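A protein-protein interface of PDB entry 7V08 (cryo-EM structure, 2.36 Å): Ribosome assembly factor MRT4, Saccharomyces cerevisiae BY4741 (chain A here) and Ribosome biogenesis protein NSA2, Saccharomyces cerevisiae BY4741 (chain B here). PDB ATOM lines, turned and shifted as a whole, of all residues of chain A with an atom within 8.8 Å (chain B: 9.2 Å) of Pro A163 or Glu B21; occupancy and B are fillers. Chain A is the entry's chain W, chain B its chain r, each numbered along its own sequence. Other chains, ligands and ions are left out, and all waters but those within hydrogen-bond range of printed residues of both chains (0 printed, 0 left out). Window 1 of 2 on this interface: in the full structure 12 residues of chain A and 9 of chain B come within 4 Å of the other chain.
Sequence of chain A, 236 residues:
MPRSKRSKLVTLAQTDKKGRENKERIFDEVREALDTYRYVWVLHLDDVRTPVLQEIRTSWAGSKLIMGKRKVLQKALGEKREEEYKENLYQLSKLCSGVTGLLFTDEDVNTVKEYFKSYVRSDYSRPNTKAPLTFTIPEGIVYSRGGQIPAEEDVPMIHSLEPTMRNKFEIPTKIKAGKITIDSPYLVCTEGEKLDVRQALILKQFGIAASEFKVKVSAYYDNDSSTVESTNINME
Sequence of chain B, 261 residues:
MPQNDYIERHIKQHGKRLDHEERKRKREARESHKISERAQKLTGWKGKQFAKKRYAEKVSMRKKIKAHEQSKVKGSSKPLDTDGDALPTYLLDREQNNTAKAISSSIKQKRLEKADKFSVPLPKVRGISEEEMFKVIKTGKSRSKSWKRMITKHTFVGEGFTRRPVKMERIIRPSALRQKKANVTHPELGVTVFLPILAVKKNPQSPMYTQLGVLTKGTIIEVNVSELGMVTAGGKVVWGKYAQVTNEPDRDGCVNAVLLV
The guanidinium group of Arg A166 sits at hydrogen-bond distance from the backbone carbonyl oxygen of Leu B18, 3.0 Å away.
O of Pro A163 sits close to ND2 of Asn A167 (3.4 Å).
The side-chain carboxylate of Glu A162 lies within salt-bridge range of the guanidinium group of Arg A166 (2.6 Å).
Pro A163 touches Glu B21 (CB to OE1, 3.9 Å).
Glu B21 touches Asn A167 (OE1 to ND2, 3.8 Å).
Ile A175 touches His B14.
Glu A162 touches none of the printed residues of chain B.
Pro A163 touches one residue of chain B.
No residue of chain B comes within 4 Å of Thr A164.
Printed residues of chain B within 4 Å of Arg A166: Leu B18.
Of the printed residues of chain B, Ile A175 touches His B14 (3.9 Å).
Lys B16 touches none of the printed residues of chain A.
Of the printed residues of chain A, Leu B18 touches Arg A166 (3.0 Å).
Glu B21 touches two residues of chain A.
Of the 17 printed residues of chain B, 3 touch a printed residue of chain A.
Printed residues of chain B that touch a printed residue of chain A: His B14, Leu B18 and Glu B21.
Printed residues of chain A that touch a printed residue of chain B: Pro A163, Arg A166, Asn A167 and Ile A175.
Hydrophobic or aromatic side chains of chain A within 4 Å of the printed part of chain B: Pro A163 and Ile A175.
Among the printed residues, 4 pairs touch across the chains.
Among the printed residues, no Asp or Glu carboxylate lies within 4 Å of a Lys or Arg side-chain nitrogen of the other chain.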
ATOM      1  N   ILE A 158     -24.858  30.867 -18.480  1.00  0.00           N
ATOM      2  CA  ILE A 158     -26.139  30.169 -18.511  1.00  0.00           C
ATOM      3  C   ILE A 158     -26.077  28.953 -17.593  1.00  0.00           C
ATOM      4  O   ILE A 158     -25.030  28.307 -17.453  1.00  0.00           O
ATOM      5  CB  ILE A 158     -26.502  29.784 -19.959  1.00  0.00           C
ATOM      6  CG1 ILE A 158     -27.912  29.188 -20.046  1.00  0.00           C
ATOM      7  CG2 ILE A 158     -25.475  28.833 -20.553  1.00  0.00           C
ATOM      8  CD1 ILE A 158     -29.024  30.191 -19.779  1.00  0.00           C
ATOM      9  N   HIS A 159     -27.199  28.654 -16.933  1.00  0.00           N
ATOM     10  CA  HIS A 159     -27.231  27.599 -15.925  1.00  0.00           C
ATOM     11  C   HIS A 159     -26.997  26.210 -16.506  1.00  0.00           C
ATOM     12  O   HIS A 159     -26.580  25.311 -15.771  1.00  0.00           O
ATOM     13  CB  HIS A 159     -28.568  27.633 -15.187  1.00  0.00           C
ATOM     14  CG  HIS A 159     -29.754  27.467 -16.084  1.00  0.00           C
ATOM     15  ND1 HIS A 159     -30.436  28.538 -16.624  1.00  0.00           N
ATOM     16  CD2 HIS A 159     -30.379  26.357 -16.539  1.00  0.00           C
ATOM     17  CE1 HIS A 159     -31.427  28.091 -17.374  1.00  0.00           C
ATOM     18  NE2 HIS A 159     -31.413  26.771 -17.340  1.00  0.00           N
ATOM     19  N   SER A 160     -27.240  26.014 -17.803  1.00  0.00           N
ATOM     20  CA  SER A 160     -27.091  24.691 -18.400  1.00  0.00           C
ATOM     21  C   SER A 160     -25.640  24.233 -18.458  1.00  0.00           C
ATOM     22  O   SER A 160     -25.388  23.047 -18.684  1.00  0.00           O
ATOM     23  CB  SER A 160     -27.691  24.676 -19.806  1.00  0.00           C
ATOM     24  OG  SER A 160     -29.021  25.160 -19.802  1.00  0.00           O
ATOM     25  N   LEU A 161     -24.685  25.139 -18.274  1.00  0.00           N
ATOM     26  CA  LEU A 161     -23.277  24.783 -18.271  1.00  0.00           C
ATOM     27  C   LEU A 161     -22.768  24.403 -16.890  1.00  0.00           C
ATOM     28  O   LEU A 161     -21.602  24.025 -16.761  1.00  0.00           O
ATOM     29  CB  LEU A 161     -22.442  25.935 -18.837  1.00  0.00           C
ATOM     30  CG  LEU A 161     -22.660  26.174 -20.329  1.00  0.00           C
ATOM     31  CD1 LEU A 161     -21.882  27.375 -20.808  1.00  0.00           C
ATOM     32  CD2 LEU A 161     -22.271  24.930 -21.121  1.00  0.00           C
ATOM     33  N   GLU A 162     -23.607  24.498 -15.863  1.00  0.00           N
ATOM     34  CA  GLU A 162     -23.174  24.114 -14.524  1.00  0.00           C
ATOM     35  C   GLU A 162     -22.818  22.636 -14.378  1.00  0.00           C
ATOM     36  O   GLU A 162     -21.787  22.355 -13.743  1.00  0.00           O
ATOM     37  CB  GLU A 162     -24.233  24.531 -13.495  1.00  0.00           C
ATOM     38  CG  GLU A 162     -23.711  24.553 -12.069  1.00  0.00           C
ATOM     39  CD  GLU A 162     -23.760  23.194 -11.408  1.00  0.00           C
ATOM     40  OE1 GLU A 162     -24.608  22.370 -11.809  1.00  0.00           O
ATOM     41  OE2 GLU A 162     -22.943  22.944 -10.501  1.00  0.00           O
ATOM     42  N   PRO A 163     -23.603  21.658 -14.865  1.00  0.00           N
ATOM     43  CA  PRO A 163     -23.138  20.263 -14.758  1.00  0.00           C
ATOM     44  C   PRO A 163     -21.853  20.003 -15.519  1.00  0.00           C
ATOM     45  O   PRO A 163     -21.019  19.208 -15.069  1.00  0.00           O
ATOM     46  CB  PRO A 163     -24.311  19.454 -15.329  1.00  0.00           C
ATOM     47  CG  PRO A 163     -25.486  20.357 -15.214  1.00  0.00           C
ATOM     48  CD  PRO A 163     -24.944  21.714 -15.475  1.00  0.00           C
ATOM     49  N   THR A 164     -21.666  20.667 -16.662  1.00  0.00           N
ATOM     50  CA  THR A 164     -20.414  20.549 -17.399  1.00  0.00           C
ATOM     51  C   THR A 164     -19.247  21.116 -16.602  1.00  0.00           C
ATOM     52  O   THR A 164     -18.171  20.513 -16.555  1.00  0.00           O
ATOM     53  CB  THR A 164     -20.538  21.256 -18.749  1.00  0.00           C
ATOM     54  OG1 THR A 164     -21.658  20.721 -19.465  1.00  0.00           O
ATOM     55  CG2 THR A 164     -19.275  21.064 -19.576  1.00  0.00           C
ATOM     56  N   MET A 165     -19.440  22.269 -15.961  1.00  0.00           N
ATOM     57  CA  MET A 165     -18.372  22.850 -15.156  1.00  0.00           C
ATOM     58  C   MET A 165     -18.071  22.008 -13.927  1.00  0.00           C
ATOM     59  O   MET A 165     -16.909  21.879 -13.533  1.00  0.00           O
ATOM     60  CB  MET A 165     -18.738  24.274 -14.739  1.00  0.00           C
ATOM     61  CG  MET A 165     -18.760  25.274 -15.879  1.00  0.00           C
ATOM     62  SD  MET A 165     -19.350  26.892 -15.362  1.00  0.00           S
ATOM     63  CE  MET A 165     -18.014  27.401 -14.289  1.00  0.00           C
ATOM     64  N   ARG A 166     -19.101  21.419 -13.321  1.00  0.00           N
ATOM     65  CA  ARG A 166     -18.925  20.650 -12.099  1.00  0.00           C
ATOM     66  C   ARG A 166     -18.259  19.305 -12.366  1.00  0.00           C
ATOM     67  O   ARG A 166     -17.315  18.931 -11.665  1.00  0.00           O
ATOM     68  CB  ARG A 166     -20.281  20.453 -11.426  1.00  0.00           C
ATOM     69  CG  ARG A 166     -20.240  20.375  -9.920  1.00  0.00           C
ATOM     70  CD  ARG A 166     -21.640  20.249  -9.342  1.00  0.00           C
ATOM     71  NE  ARG A 166     -22.301  19.016  -9.752  1.00  0.00           N
ATOM     72  CZ  ARG A 166     -23.420  18.952 -10.462  1.00  0.00           C
ATOM     73  NH1 ARG A 166     -24.055  20.040 -10.857  1.00  0.00           N
ATOM     74  NH2 ARG A 166     -23.917  17.761 -10.779  1.00  0.00           N
ATOM     75  N   ASN A 167     -18.712  18.576 -13.385  1.00  0.00           N
ATOM     76  CA  ASN A 167     -18.212  17.230 -13.643  1.00  0.00           C
ATOM     77  C   ASN A 167     -17.010  17.228 -14.582  1.00  0.00           C
ATOM     78  O   ASN A 167     -15.946  16.715 -14.229  1.00  0.00           O
ATOM     79  CB  ASN A 167     -19.333  16.352 -14.215  1.00  0.00           C
ATOM     80  CG  ASN A 167     -20.561  16.325 -13.331  1.00  0.00           C
ATOM     81  OD1 ASN A 167     -20.481  16.546 -12.124  1.00  0.00           O
ATOM     82  ND2 ASN A 167     -21.711  16.052 -13.933  1.00  0.00           N
ATOM     83  N   LYS A 168     -17.164  17.794 -15.779  1.00  0.00           N
ATOM     84  CA  LYS A 168     -16.111  17.688 -16.784  1.00  0.00           C
ATOM     85  C   LYS A 168     -14.889  18.524 -16.423  1.00  0.00           C
ATOM     86  O   LYS A 168     -13.758  18.028 -16.483  1.00  0.00           O
ATOM     87  CB  LYS A 168     -16.656  18.089 -18.153  1.00  0.00           C
ATOM     88  CG  LYS A 168     -15.581  18.451 -19.162  1.00  0.00           C
ATOM     89  CD  LYS A 168     -16.105  18.384 -20.580  1.00  0.00           C
ATOM     90  CE  LYS A 168     -16.052  16.963 -21.096  1.00  0.00           C
ATOM     91  NZ  LYS A 168     -14.654  16.437 -21.129  1.00  0.00           N
ATOM     92  N   PHE A 169     -15.084  19.786 -16.041  1.00  0.00           N
ATOM     93  CA  PHE A 169     -13.958  20.649 -15.702  1.00  0.00           C
ATOM     94  C   PHE A 169     -13.504  20.499 -14.256  1.00  0.00           C
ATOM     95  O   PHE A 169     -12.446  21.033 -13.905  1.00  0.00           O
ATOM     96  CB  PHE A 169     -14.296  22.125 -15.949  1.00  0.00           C
ATOM     97  CG  PHE A 169     -14.729  22.440 -17.358  1.00  0.00           C
ATOM     98  CD1 PHE A 169     -14.342  21.648 -18.425  1.00  0.00           C
ATOM     99  CD2 PHE A 169     -15.522  23.545 -17.611  1.00  0.00           C
ATOM    100  CE1 PHE A 169     -14.755  21.942 -19.709  1.00  0.00           C
ATOM    101  CE2 PHE A 169     -15.930  23.851 -18.893  1.00  0.00           C
ATOM    102  CZ  PHE A 169     -15.548  23.048 -19.943  1.00  0.00           C
ATOM    103  N   GLU A 170     -14.279  19.804 -13.420  1.00  0.00           N
ATOM    104  CA  GLU A 170     -13.978  19.621 -11.997  1.00  0.00           C
ATOM    105  C   GLU A 170     -13.803  20.958 -11.277  1.00  0.00           C
ATOM    106  O   GLU A 170     -12.847  21.156 -10.524  1.00  0.00           O
ATOM    107  CB  GLU A 170     -12.747  18.730 -11.805  1.00  0.00           C
ATOM    108  CG  GLU A 170     -12.827  17.416 -12.566  1.00  0.00           C
ATOM    109  CD  GLU A 170     -11.549  16.602 -12.492  1.00  0.00           C
ATOM    110  OE1 GLU A 170     -10.690  16.896 -11.631  1.00  0.00           O
ATOM    111  OE2 GLU A 170     -11.406  15.659 -13.298  1.00  0.00           O
ATOM    112  N   ILE A 171     -14.721  21.884 -11.516  1.00  0.00           N
ATOM    113  CA  ILE A 171     -14.730  23.196 -10.871  1.00  0.00           C
ATOM    114  C   ILE A 171     -15.837  23.207  -9.823  1.00  0.00           C
ATOM    115  O   ILE A 171     -16.983  22.879 -10.149  1.00  0.00           O
ATOM    116  CB  ILE A 171     -14.942  24.339 -11.881  1.00  0.00           C
ATOM    117  CG1 ILE A 171     -13.854  24.330 -12.952  1.00  0.00           C
ATOM    118  CG2 ILE A 171     -14.942  25.675 -11.168  1.00  0.00           C
ATOM    119  CD1 ILE A 171     -14.035  25.392 -14.009  1.00  0.00           C
ATOM    120  N   THR A 173     -18.774  24.420  -8.248  1.00  0.00           N
ATOM    121  CA  THR A 173     -19.776  25.420  -8.576  1.00  0.00           C
ATOM    122  C   THR A 173     -21.097  25.053  -7.925  1.00  0.00           C
ATOM    123  O   THR A 173     -21.386  23.876  -7.693  1.00  0.00           O
ATOM    124  CB  THR A 173     -19.976  25.549 -10.093  1.00  0.00           C
ATOM    125  OG1 THR A 173     -20.302  24.267 -10.640  1.00  0.00           O
ATOM    126  CG2 THR A 173     -18.715  26.070 -10.763  1.00  0.00           C
ATOM    127  N   LYS A 174     -21.896  26.073  -7.627  1.00  0.00           N
ATOM    128  CA  LYS A 174     -23.231  25.883  -7.086  1.00  0.00           C
ATOM    129  C   LYS A 174     -24.199  26.818  -7.799  1.00  0.00           C
ATOM    130  O   LYS A 174     -23.840  27.919  -8.215  1.00  0.00           O
ATOM    131  CB  LYS A 174     -23.270  26.126  -5.565  1.00  0.00           C
ATOM    132  CG  LYS A 174     -22.524  25.085  -4.723  1.00  0.00           C
ATOM    133  CD  LYS A 174     -21.054  25.448  -4.521  1.00  0.00           C
ATOM    134  CE  LYS A 174     -20.267  24.298  -3.918  1.00  0.00           C
ATOM    135  NZ  LYS A 174     -18.809  24.602  -3.825  1.00  0.00           N
ATOM    136  N   ILE A 175     -25.446  26.382  -7.922  1.00  0.00           N
ATOM    137  CA  ILE A 175     -26.482  27.177  -8.570  1.00  0.00           C
ATOM    138  C   ILE A 175     -27.248  27.914  -7.484  1.00  0.00           C
ATOM    139  O   ILE A 175     -27.868  27.294  -6.612  1.00  0.00           O
ATOM    140  CB  ILE A 175     -27.419  26.324  -9.432  1.00  0.00           C
ATOM    141  CG1 ILE A 175     -26.699  25.872 -10.696  1.00  0.00           C
ATOM    142  CG2 ILE A 175     -28.659  27.120  -9.811  1.00  0.00           C
ATOM    143  CD1 ILE A 175     -27.591  25.174 -11.705  1.00  0.00           C
ATOM    144  N   ILE A 180     -24.548  30.511 -11.764  1.00  0.00           N
ATOM    145  CA  ILE A 180     -23.412  29.704 -11.344  1.00  0.00           C
ATOM    146  C   ILE A 180     -22.512  30.553 -10.461  1.00  0.00           C
ATOM    147  O   ILE A 180     -22.099  31.653 -10.851  1.00  0.00           O
ATOM    148  CB  ILE A 180     -22.653  29.158 -12.562  1.00  0.00           C
ATOM    149  CG1 ILE A 180     -23.575  28.280 -13.407  1.00  0.00           C
ATOM    150  CG2 ILE A 180     -21.422  28.384 -12.132  1.00  0.00           C
ATOM    151  CD1 ILE A 180     -22.956  27.799 -14.686  1.00  0.00           C
ATOM    152  N   ILE B  11     -36.077  23.731 -11.733  1.00  0.00           N
ATOM    153  CA  ILE B  11     -34.846  23.191 -12.301  1.00  0.00           C
ATOM    154  C   ILE B  11     -33.965  24.323 -12.808  1.00  0.00           C
ATOM    155  O   ILE B  11     -32.743  24.310 -12.622  1.00  0.00           O
ATOM    156  CB  ILE B  11     -35.165  22.168 -13.406  1.00  0.00           C
ATOM    157  CG1 ILE B  11     -35.909  20.968 -12.814  1.00  0.00           C
ATOM    158  CG2 ILE B  11     -33.893  21.706 -14.098  1.00  0.00           C
ATOM    159  CD1 ILE B  11     -36.232  19.894 -13.811  1.00  0.00           C
ATOM    160  N   HIS B  14     -32.526  26.041  -9.536  1.00  0.00           N
ATOM    161  CA  HIS B  14     -31.821  25.233  -8.550  1.00  0.00           C
ATOM    162  C   HIS B  14     -31.054  24.060  -9.132  1.00  0.00           C
ATOM    163  O   HIS B  14     -30.234  23.478  -8.416  1.00  0.00           O
ATOM    164  CB  HIS B  14     -32.798  24.686  -7.497  1.00  0.00           C
ATOM    165  CG  HIS B  14     -33.518  25.747  -6.731  1.00  0.00           C
ATOM    166  ND1 HIS B  14     -32.905  26.509  -5.763  1.00  0.00           N
ATOM    167  CD2 HIS B  14     -34.798  26.183  -6.799  1.00  0.00           C
ATOM    168  CE1 HIS B  14     -33.776  27.366  -5.264  1.00  0.00           C
ATOM    169  NE2 HIS B  14     -34.932  27.189  -5.876  1.00  0.00           N
ATOM    170  N   GLY B  15     -31.284  23.693 -10.380  1.00  0.00           N
ATOM    171  CA  GLY B  15     -30.623  22.547 -10.953  1.00  0.00           C
ATOM    172  C   GLY B  15     -31.308  21.248 -10.577  1.00  0.00           C
ATOM    173  O   GLY B  15     -32.454  21.203 -10.136  1.00  0.00           O
ATOM    174  N   LYS B  16     -30.574  20.166 -10.775  1.00  0.00           N
ATOM    175  CA  LYS B  16     -31.045  18.827 -10.467  1.00  0.00           C
ATOM    176  C   LYS B  16     -30.181  18.231  -9.362  1.00  0.00           C
ATOM    177  O   LYS B  16     -29.261  18.871  -8.857  1.00  0.00           O
ATOM    178  CB  LYS B  16     -31.031  17.958 -11.725  1.00  0.00           C
ATOM    179  CG  LYS B  16     -31.867  18.510 -12.855  1.00  0.00           C
ATOM    180  CD  LYS B  16     -31.976  17.519 -13.985  1.00  0.00           C
ATOM    181  CE  LYS B  16     -32.893  18.028 -15.073  1.00  0.00           C
ATOM    182  NZ  LYS B  16     -32.690  17.270 -16.336  1.00  0.00           N
ATOM    183  N   ARG B  17     -30.488  16.992  -8.987  1.00  0.00           N
ATOM    184  CA  ARG B  17     -29.642  16.275  -8.045  1.00  0.00           C
ATOM    185  C   ARG B  17     -28.261  16.068  -8.653  1.00  0.00           C
ATOM    186  O   ARG B  17     -28.112  15.925  -9.869  1.00  0.00           O
ATOM    187  CB  ARG B  17     -30.283  14.937  -7.660  1.00  0.00           C
ATOM    188  CG  ARG B  17     -31.509  15.094  -6.770  1.00  0.00           C
ATOM    189  CD  ARG B  17     -32.247  13.789  -6.528  1.00  0.00           C
ATOM    190  NE  ARG B  17     -31.566  12.916  -5.581  1.00  0.00           N
ATOM    191  CZ  ARG B  17     -31.769  12.927  -4.271  1.00  0.00           C
ATOM    192  NH1 ARG B  17     -32.607  13.785  -3.709  1.00  0.00           N
ATOM    193  NH2 ARG B  17     -31.109  12.064  -3.505  1.00  0.00           N
ATOM    194  N   LEU B  18     -27.240  16.093  -7.796  1.00  0.00           N
ATOM    195  CA  LEU B  18     -25.865  16.150  -8.284  1.00  0.00           C
ATOM    196  C   LEU B  18     -25.468  14.900  -9.062  1.00  0.00           C
ATOM    197  O   LEU B  18     -24.515  14.947  -9.845  1.00  0.00           O
ATOM    198  CB  LEU B  18     -24.898  16.373  -7.123  1.00  0.00           C
ATOM    199  CG  LEU B  18     -25.012  17.683  -6.338  1.00  0.00           C
ATOM    200  CD1 LEU B  18     -23.909  17.791  -5.311  1.00  0.00           C
ATOM    201  CD2 LEU B  18     -24.998  18.892  -7.255  1.00  0.00           C
ATOM    202  N   ASP B  19     -26.175  13.784  -8.875  1.00  0.00           N
ATOM    203  CA  ASP B  19     -25.863  12.546  -9.579  1.00  0.00           C
ATOM    204  C   ASP B  19     -26.847  12.244 -10.704  1.00  0.00           C
ATOM    205  O   ASP B  19     -26.926  11.098 -11.154  1.00  0.00           O
ATOM    206  CB  ASP B  19     -25.807  11.377  -8.595  1.00  0.00           C
ATOM    207  CG  ASP B  19     -27.160  11.054  -7.973  1.00  0.00           C
ATOM    208  OD1 ASP B  19     -28.082  11.894  -8.023  1.00  0.00           O
ATOM    209  OD2 ASP B  19     -27.291   9.953  -7.409  1.00  0.00           O
ATOM    210  N   HIS B  20     -27.596  13.247 -11.162  1.00  0.00           N
ATOM    211  CA  HIS B  20     -28.690  12.990 -12.091  1.00  0.00           C
ATOM    212  C   HIS B  20     -28.183  12.471 -13.430  1.00  0.00           C
ATOM    213  O   HIS B  20     -28.643  11.433 -13.920  1.00  0.00           O
ATOM    214  CB  HIS B  20     -29.512  14.258 -12.293  1.00  0.00           C
ATOM    215  CG  HIS B  20     -30.667  14.073 -13.223  1.00  0.00           C
ATOM    216  ND1 HIS B  20     -30.598  14.382 -14.563  1.00  0.00           N
ATOM    217  CD2 HIS B  20     -31.910  13.585 -13.010  1.00  0.00           C
ATOM    218  CE1 HIS B  20     -31.755  14.106 -15.135  1.00  0.00           C
ATOM    219  NE2 HIS B  20     -32.568  13.620 -14.214  1.00  0.00           N
ATOM    220  N   GLU B  21     -27.228  13.184 -14.034  1.00  0.00           N
ATOM    221  CA  GLU B  21     -26.742  12.811 -15.358  1.00  0.00           C
ATOM    222  C   GLU B  21     -26.051  11.457 -15.326  1.00  0.00           C
ATOM    223  O   GLU B  21     -26.289  10.604 -16.186  1.00  0.00           O
ATOM    224  CB  GLU B  21     -25.783  13.871 -15.899  1.00  0.00           C
ATOM    225  CG  GLU B  21     -26.389  15.231 -16.130  1.00  0.00           C
ATOM    226  CD  GLU B  21     -26.409  16.084 -14.883  1.00  0.00           C
ATOM    227  OE1 GLU B  21     -25.472  15.960 -14.060  1.00  0.00           O
ATOM    228  OE2 GLU B  21     -27.363  16.875 -14.726  1.00  0.00           O
ATOM    229  N   GLU B  22     -25.194  11.244 -14.329  1.00  0.00           N
ATOM    230  CA  GLU B  22     -24.456   9.992 -14.243  1.00  0.00           C
ATOM    231  C   GLU B  22     -25.388   8.817 -13.997  1.00  0.00           C
ATOM    232  O   GLU B  22     -25.244   7.758 -14.616  1.00  0.00           O
ATOM    233  CB  GLU B  22     -23.403  10.088 -13.141  1.00  0.00           C
ATOM    234  CG  GLU B  22     -22.497   8.887 -13.059  1.00  0.00           C
ATOM    235  CD  GLU B  22     -21.662   8.695 -14.313  1.00  0.00           C
ATOM    236  OE1 GLU B  22     -21.335   9.693 -14.988  1.00  0.00           O
ATOM    237  OE2 GLU B  22     -21.333   7.535 -14.630  1.00  0.00           O
ATOM    238  N   ARG B  23     -26.361   8.994 -13.106  1.00  0.00           N
ATOM    239  CA  ARG B  23     -27.301   7.925 -12.800  1.00  0.00           C
ATOM    240  C   ARG B  23     -28.161   7.575 -14.012  1.00  0.00           C
ATOM    241  O   ARG B  23     -28.382   6.393 -14.309  1.00  0.00           O
ATOM    242  CB  ARG B  23     -28.160   8.351 -11.617  1.00  0.00           C
ATOM    243  CG  ARG B  23     -28.584   7.236 -10.736  1.00  0.00           C
ATOM    244  CD  ARG B  23     -28.834   7.725  -9.331  1.00  0.00           C
ATOM    245  NE  ARG B  23     -29.635   6.763  -8.585  1.00  0.00           N
ATOM    246  CZ  ARG B  23     -30.960   6.766  -8.557  1.00  0.00           C
ATOM    247  NH1 ARG B  23     -31.661   7.667  -9.223  1.00  0.00           N
ATOM    248  NH2 ARG B  23     -31.595   5.844  -7.842  1.00  0.00           N
ATOM    249  N   LYS B  24     -28.635   8.593 -14.733  1.00  0.00           N
ATOM    250  CA  LYS B  24     -29.412   8.365 -15.949  1.00  0.00           C
ATOM    251  C   LYS B  24     -28.576   7.676 -17.025  1.00  0.00           C
ATOM    252  O   LYS B  24     -29.054   6.763 -17.712  1.00  0.00           O
ATOM    253  CB  LYS B  24     -29.955   9.707 -16.436  1.00  0.00           C
ATOM    254  CG  LYS B  24     -30.672   9.707 -17.763  1.00  0.00           C
ATOM    255  CD  LYS B  24     -31.108  11.129 -18.078  1.00  0.00           C
ATOM    256  CE  LYS B  24     -31.882  11.222 -19.372  1.00  0.00           C
ATOM    257  NZ  LYS B  24     -31.050  10.860 -20.550  1.00  0.00           N
ATOM    258  N   ARG B  25     -27.314   8.088 -17.163  1.00  0.00           N
ATOM    259  CA  ARG B  25     -26.410   7.489 -18.135  1.00  0.00           C
ATOM    260  C   ARG B  25     -26.145   6.017 -17.832  1.00  0.00           C
ATOM    261  O   ARG B  25     -26.155   5.176 -18.739  1.00  0.00           O
ATOM    262  CB  ARG B  25     -25.106   8.275 -18.142  1.00  0.00           C
ATOM    263  CG  ARG B  25     -24.428   8.368 -19.486  1.00  0.00           C
ATOM    264  CD  ARG B  25     -23.246   7.453 -19.534  1.00  0.00           C
ATOM    265  NE  ARG B  25     -22.367   7.652 -18.391  1.00  0.00           N
ATOM    266  CZ  ARG B  25     -21.621   6.696 -17.858  1.00  0.00           C
ATOM    267  NH1 ARG B  25     -21.605   5.475 -18.359  1.00  0.00           N
ATOM    268  NH2 ARG B  25     -20.868   6.974 -16.800  1.00  0.00           N
ATOM    269  N   LYS B  26     -25.915   5.684 -16.563  1.00  0.00           N
ATOM    270  CA  LYS B  26     -25.673   4.292 -16.205  1.00  0.00           C
ATOM    271  C   LYS B  26     -26.934   3.447 -16.356  1.00  0.00           C
ATOM    272  O   LYS B  26     -26.849   2.275 -16.733  1.00  0.00           O
ATOM    273  CB  LYS B  26     -25.113   4.200 -14.789  1.00  0.00           C
ATOM    274  CG  LYS B  26     -23.775   4.890 -14.627  1.00  0.00           C
ATOM    275  CD  LYS B  26     -23.139   4.614 -13.281  1.00  0.00           C
ATOM    276  CE  LYS B  26     -22.506   3.237 -13.249  1.00  0.00           C
ATOM    277  NZ  LYS B  26     -21.602   3.037 -12.094  1.00  0.00           N
ATOM    278  N   ARG B  27     -28.113   4.022 -16.090  1.00  0.00           N
ATOM    279  CA  ARG B  27     -29.356   3.287 -16.322  1.00  0.00           C
ATOM    280  C   ARG B  27     -29.549   2.972 -17.806  1.00  0.00           C
ATOM    281  O   ARG B  27     -29.886   1.836 -18.173  1.00  0.00           O
ATOM    282  CB  ARG B  27     -30.541   4.082 -15.774  1.00  0.00           C
ATOM    283  CG  ARG B  27     -31.878   3.371 -15.897  1.00  0.00           C
ATOM    284  CD  ARG B  27     -32.970   4.062 -15.098  1.00  0.00           C
ATOM    285  NE  ARG B  27     -33.315   5.373 -15.635  1.00  0.00           N
ATOM    286  CZ  ARG B  27     -32.974   6.531 -15.085  1.00  0.00           C
ATOM    287  NH1 ARG B  27     -32.271   6.585 -13.964  1.00  0.00           N
ATOM    288  NH2 ARG B  27     -33.360   7.662 -15.666  1.00  0.00           N
ATOM    289  N   GLU B  28     -29.296   3.957 -18.673  1.00  0.00           N
ATOM    290  CA  GLU B  28     -29.386   3.723 -20.113  1.00  0.00           C
ATOM    291  C   GLU B  28     -28.356   2.707 -20.591  1.00  0.00           C
ATOM    292  O   GLU B  28     -28.647   1.920 -21.496  1.00  0.00           O
ATOM    293  CB  GLU B  28     -29.221   5.035 -20.874  1.00  0.00           C
ATOM    294  CG  GLU B  28     -30.335   6.024 -20.619  1.00  0.00           C
ATOM    295  CD  GLU B  28     -30.026   7.414 -21.130  1.00  0.00           C
ATOM    296  OE1 GLU B  28     -28.867   7.678 -21.505  1.00  0.00           O
ATOM    297  OE2 GLU B  28     -30.956   8.248 -21.156  1.00  0.00           O
ATOM    298  N   ALA B  29     -27.157   2.705 -20.005  1.00  0.00           N
ATOM    299  CA  ALA B  29     -26.170   1.692 -20.366  1.00  0.00           C
ATOM    300  C   ALA B  29     -26.590   0.305 -19.889  1.00  0.00           C
ATOM    301  O   ALA B  29     -26.315  -0.697 -20.558  1.00  0.00           O
ATOM    302  CB  ALA B  29     -24.804   2.059 -19.799  1.00  0.00           C
